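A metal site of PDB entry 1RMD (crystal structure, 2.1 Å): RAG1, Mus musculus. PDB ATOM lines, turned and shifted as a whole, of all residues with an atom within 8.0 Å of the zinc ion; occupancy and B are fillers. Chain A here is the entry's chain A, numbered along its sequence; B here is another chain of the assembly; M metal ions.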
ATOM      1  N   THR A  39     -31.470 -21.514  11.543  1.00  0.00           N
ATOM      2  CA  THR A  39     -30.418 -20.884  10.766  1.00  0.00           C
ATOM      3  C   THR A  39     -31.028 -20.314   9.490  1.00  0.00           C
ATOM      4  O   THR A  39     -32.145 -20.697   9.117  1.00  0.00           O
ATOM      5  CB  THR A  39     -29.317 -21.893  10.356  1.00  0.00           C
ATOM      6  OG1 THR A  39     -29.868 -22.895   9.486  1.00  0.00           O
ATOM      7  CG2 THR A  39     -28.707 -22.544  11.583  1.00  0.00           C
ATOM      8  N   SER A  40     -30.295 -19.434   8.810  1.00  0.00           N
ATOM      9  CA  SER A  40     -30.773 -18.829   7.561  1.00  0.00           C
ATOM     10  C   SER A  40     -31.142 -19.952   6.570  1.00  0.00           C
ATOM     11  O   SER A  40     -32.141 -19.861   5.838  1.00  0.00           O
ATOM     12  CB  SER A  40     -29.689 -17.904   6.987  1.00  0.00           C
ATOM     13  OG  SER A  40     -29.422 -16.834   7.894  1.00  0.00           O
ATOM     14  N   CYS A  41     -30.393 -21.051   6.659  1.00  0.00           N
ATOM     15  CA  CYS A  41     -30.613 -22.210   5.791  1.00  0.00           C
ATOM     16  C   CYS A  41     -31.737 -23.169   6.261  1.00  0.00           C
ATOM     17  O   CYS A  41     -31.819 -24.299   5.790  1.00  0.00           O
ATOM     18  CB  CYS A  41     -29.289 -22.953   5.578  1.00  0.00           C
ATOM     19  SG  CYS A  41     -28.334 -23.243   7.091  1.00  0.00           S
ATOM     20  N   LYS A  42     -32.590 -22.702   7.173  1.00  0.00           N
ATOM     21  CA  LYS A  42     -33.741 -23.467   7.659  1.00  0.00           C
ATOM     22  C   LYS A  42     -33.458 -24.760   8.425  1.00  0.00           C
ATOM     23  O   LYS A  42     -34.253 -25.700   8.387  1.00  0.00           O
ATOM     24  CB  LYS A  42     -34.707 -23.788   6.510  1.00  0.00           C
ATOM     25  CG  LYS A  42     -35.045 -22.607   5.610  1.00  0.00           C
ATOM     26  CD  LYS A  42     -36.241 -21.838   6.088  1.00  0.00           C
ATOM     27  CE  LYS A  42     -36.631 -20.811   5.051  1.00  0.00           C
ATOM     28  NZ  LYS A  42     -36.813 -21.433   3.682  1.00  0.00           N
ATOM     29  N   HIS A  43     -32.336 -24.826   9.097  1.00  0.00           N
ATOM     30  CA  HIS A  43     -32.005 -25.997   9.872  1.00  0.00           C
ATOM     31  C   HIS A  43     -32.159 -25.679  11.362  1.00  0.00           C
ATOM     32  O   HIS A  43     -31.941 -24.544  11.791  1.00  0.00           O
ATOM     33  CB  HIS A  43     -30.598 -26.419   9.521  1.00  0.00           C
ATOM     34  CG  HIS A  43     -30.487 -26.934   8.133  1.00  0.00           C
ATOM     35  ND1 HIS A  43     -29.605 -26.395   7.235  1.00  0.00           N
ATOM     36  CD2 HIS A  43     -31.172 -27.921   7.534  1.00  0.00           C
ATOM     37  CE1 HIS A  43     -29.773 -27.072   6.120  1.00  0.00           C
ATOM     38  NE2 HIS A  43     -30.715 -28.018   6.259  1.00  0.00           N
ATOM     39  N   LEU A  44     -32.519 -26.688  12.158  1.00  0.00           N
ATOM     40  CA  LEU A  44     -32.747 -26.502  13.592  1.00  0.00           C
ATOM     41  C   LEU A  44     -31.706 -27.055  14.579  1.00  0.00           C
ATOM     42  O   LEU A  44     -31.130 -28.126  14.353  1.00  0.00           O
ATOM     43  CB  LEU A  44     -34.136 -27.050  13.948  1.00  0.00           C
ATOM     44  CG  LEU A  44     -35.305 -26.462  13.144  1.00  0.00           C
ATOM     45  CD1 LEU A  44     -36.593 -27.029  13.613  1.00  0.00           C
ATOM     46  CD2 LEU A  44     -35.326 -24.944  13.264  1.00  0.00           C
ATOM     47  N   PHE A  45     -31.456 -26.314  15.657  1.00  0.00           N
ATOM     48  CA  PHE A  45     -30.503 -26.699  16.726  1.00  0.00           C
ATOM     49  C   PHE A  45     -30.930 -26.019  18.026  1.00  0.00           C
ATOM     50  O   PHE A  45     -31.499 -24.924  17.998  1.00  0.00           O
ATOM     51  CB  PHE A  45     -29.072 -26.221  16.436  1.00  0.00           C
ATOM     52  CG  PHE A  45     -28.599 -26.520  15.071  1.00  0.00           C
ATOM     53  CD1 PHE A  45     -28.851 -25.636  14.025  1.00  0.00           C
ATOM     54  CD2 PHE A  45     -27.945 -27.715  14.793  1.00  0.00           C
ATOM     55  CE1 PHE A  45     -28.471 -25.933  12.716  1.00  0.00           C
ATOM     56  CE2 PHE A  45     -27.552 -28.030  13.482  1.00  0.00           C
ATOM     57  CZ  PHE A  45     -27.824 -27.117  12.435  1.00  0.00           C
ATOM     58  N   TYR A  60     -20.038 -21.927  10.135  1.00  0.00           N
ATOM     59  CA  TYR A  60     -20.687 -22.735   9.110  1.00  0.00           C
ATOM     60  C   TYR A  60     -21.735 -23.666   9.742  1.00  0.00           C
ATOM     61  O   TYR A  60     -21.522 -24.171  10.847  1.00  0.00           O
ATOM     62  CB  TYR A  60     -19.651 -23.574   8.388  1.00  0.00           C
ATOM     63  CG  TYR A  60     -18.713 -22.742   7.576  1.00  0.00           C
ATOM     64  CD1 TYR A  60     -19.170 -22.029   6.470  1.00  0.00           C
ATOM     65  CD2 TYR A  60     -17.374 -22.670   7.908  1.00  0.00           C
ATOM     66  CE1 TYR A  60     -18.307 -21.253   5.708  1.00  0.00           C
ATOM     67  CE2 TYR A  60     -16.489 -21.893   7.164  1.00  0.00           C
ATOM     68  CZ  TYR A  60     -16.962 -21.195   6.079  1.00  0.00           C
ATOM     69  OH  TYR A  60     -16.078 -20.438   5.359  1.00  0.00           O
ATOM     70  N   CYS A  61     -22.830 -23.895   9.029  1.00  0.00           N
ATOM     71  CA  CYS A  61     -23.918 -24.749   9.515  1.00  0.00           C
ATOM     72  C   CYS A  61     -23.488 -26.199   9.617  1.00  0.00           C
ATOM     73  O   CYS A  61     -23.010 -26.786   8.647  1.00  0.00           O
ATOM     74  CB  CYS A  61     -25.131 -24.692   8.576  1.00  0.00           C
ATOM     75  SG  CYS A  61     -26.465 -25.822   9.036  1.00  0.00           S
ATOM     76  N   PRO A  62     -23.682 -26.814  10.801  1.00  0.00           N
ATOM     77  CA  PRO A  62     -23.289 -28.221  10.978  1.00  0.00           C
ATOM     78  C   PRO A  62     -23.991 -29.164   9.974  1.00  0.00           C
ATOM     79  O   PRO A  62     -23.411 -30.163   9.560  1.00  0.00           O
ATOM     80  CB  PRO A  62     -23.712 -28.507  12.411  1.00  0.00           C
ATOM     81  CG  PRO A  62     -23.675 -27.163  13.073  1.00  0.00           C
ATOM     82  CD  PRO A  62     -24.280 -26.283  12.031  1.00  0.00           C
ATOM     83  N   SER A  63     -25.225 -28.820   9.592  1.00  0.00           N
ATOM     84  CA  SER A  63     -26.000 -29.633   8.654  1.00  0.00           C
ATOM     85  C   SER A  63     -25.546 -29.510   7.209  1.00  0.00           C
ATOM     86  O   SER A  63     -25.206 -30.523   6.575  1.00  0.00           O
ATOM     87  CB  SER A  63     -27.477 -29.260   8.695  1.00  0.00           C
ATOM     88  OG  SER A  63     -28.082 -29.611   9.930  1.00  0.00           O
ATOM     89  N   CYS A  64     -25.518 -28.277   6.706  1.00  0.00           N
ATOM     90  CA  CYS A  64     -25.154 -28.049   5.306  1.00  0.00           C
ATOM     91  C   CYS A  64     -23.842 -27.345   4.985  1.00  0.00           C
ATOM     92  O   CYS A  64     -23.448 -27.278   3.818  1.00  0.00           O
ATOM     93  CB  CYS A  64     -26.306 -27.373   4.575  1.00  0.00           C
ATOM     94  SG  CYS A  64     -26.700 -25.754   5.168  1.00  0.00           S
ATOM     95  N   ARG A  65     -23.194 -26.799   6.010  1.00  0.00           N
ATOM     96  CA  ARG A  65     -21.895 -26.116   5.862  1.00  0.00           C
ATOM     97  C   ARG A  65     -21.945 -24.766   5.187  1.00  0.00           C
ATOM     98  O   ARG A  65     -20.934 -24.269   4.670  1.00  0.00           O
ATOM     99  CB  ARG A  65     -20.891 -27.011   5.104  1.00  0.00           C
ATOM    100  CG  ARG A  65     -20.486 -28.312   5.813  1.00  0.00           C
ATOM    101  CD  ARG A  65     -19.866 -29.311   4.828  1.00  0.00           C
ATOM    102  NE  ARG A  65     -20.883 -29.833   3.902  1.00  0.00           N
ATOM    103  CZ  ARG A  65     -20.867 -29.677   2.573  1.00  0.00           C
ATOM    104  NH1 ARG A  65     -19.887 -29.017   1.946  1.00  0.00           N
ATOM    105  NH2 ARG A  65     -21.872 -30.172   1.841  1.00  0.00           N
ATOM    106  N   TYR A  66     -23.129 -24.157   5.165  1.00  0.00           N
ATOM    107  CA  TYR A  66     -23.310 -22.837   4.551  1.00  0.00           C
ATOM    108  C   TYR A  66     -22.987 -21.822   5.662  1.00  0.00           C
ATOM    109  O   TYR A  66     -23.301 -22.054   6.825  1.00  0.00           O
ATOM    110  CB  TYR A  66     -24.769 -22.701   4.080  1.00  0.00           C
ATOM    111  CG  TYR A  66     -25.053 -21.681   3.005  1.00  0.00           C
ATOM    112  CD1 TYR A  66     -24.505 -21.803   1.735  1.00  0.00           C
ATOM    113  CD2 TYR A  66     -25.922 -20.595   3.251  1.00  0.00           C
ATOM    114  CE1 TYR A  66     -24.795 -20.868   0.719  1.00  0.00           C
ATOM    115  CE2 TYR A  66     -26.225 -19.663   2.263  1.00  0.00           C
ATOM    116  CZ  TYR A  66     -25.664 -19.803   0.989  1.00  0.00           C
ATOM    117  OH  TYR A  66     -25.941 -18.873  -0.009  1.00  0.00           O
ATOM    118  N   PRO A  67     -22.288 -20.712   5.325  1.00  0.00           N
ATOM    119  CA  PRO A  67     -21.929 -19.697   6.326  1.00  0.00           C
ATOM    120  C   PRO A  67     -23.058 -19.425   7.320  1.00  0.00           C
ATOM    121  O   PRO A  67     -24.199 -19.212   6.924  1.00  0.00           O
ATOM    122  CB  PRO A  67     -21.595 -18.486   5.467  1.00  0.00           C
ATOM    123  CG  PRO A  67     -20.983 -19.126   4.252  1.00  0.00           C
ATOM    124  CD  PRO A  67     -21.902 -20.276   3.970  1.00  0.00           C
ATOM    125  N   CYS A  68     -22.732 -19.470   8.616  1.00  0.00           N
ATOM    126  CA  CYS A  68     -23.710 -19.298   9.669  1.00  0.00           C
ATOM    127  C   CYS A  68     -23.221 -18.441  10.848  1.00  0.00           C
ATOM    128  O   CYS A  68     -22.202 -18.738  11.463  1.00  0.00           O
ATOM    129  CB  CYS A  68     -24.116 -20.692  10.176  1.00  0.00           C
ATOM    130  SG  CYS A  68     -25.473 -20.714  11.358  1.00  0.00           S
ATOM    131  N   HIS B  19     -36.243 -29.648   7.392  1.00  0.00           N
ATOM    132  CA  HIS B  19     -36.353 -31.059   7.743  1.00  0.00           C
ATOM    133  C   HIS B  19     -37.809 -31.429   8.009  1.00  0.00           C
ATOM    134  O   HIS B  19     -38.225 -32.541   7.695  1.00  0.00           O
ATOM    135  CB  HIS B  19     -35.417 -31.444   8.866  1.00  0.00           C
ATOM    136  CG  HIS B  19     -33.958 -31.430   8.482  1.00  0.00           C
ATOM    137  ND1 HIS B  19     -33.511 -31.724   7.213  1.00  0.00           N
ATOM    138  CD2 HIS B  19     -32.840 -31.130   9.205  1.00  0.00           C
ATOM    139  CE1 HIS B  19     -32.188 -31.612   7.163  1.00  0.00           C
ATOM    140  NE2 HIS B  19     -31.767 -31.256   8.365  1.00  0.00           N
HETATM  141 ZN    ZN M   1     -27.717 -25.531   7.161  1.00  0.00          ZN
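ND1 of His 43 is bound to the zinc ion, 2.1 Å away.
The zinc ion is bound by SG of Cys 64 (2.2 Å).
SG of Cys 61 binds the zinc ion (2.3 Å).
SG of Cys 41 binds the zinc ion (2.4 Å).
The zinc ion has four donor atoms within binding distance.
Within 4 Å of the zinc ion: Cys 41, His 43, Cys 61 and Cys 64.
The nearest printed residue that does not touch the zinc ion is Ser 63 (4.04 Å).
The side-chain hydroxyl (OG1) of Thr 39 sits close to the backbone NH (N) of Cys 41, 3.4 Å away.
The backbone NH (N) of Ser 63 lies close to the side-chain sulfur (SG) of Cys 61, 3.3 Å away.
The backbone NH (N) of Cys 61 sits at hydrogen-bond distance from the backbone carbonyl oxygen (O) of Tyr 66 (2.9 Å).
N of His 43 is in hydrogen-bond range of OG1 of Thr 39, 3.2 Å away.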
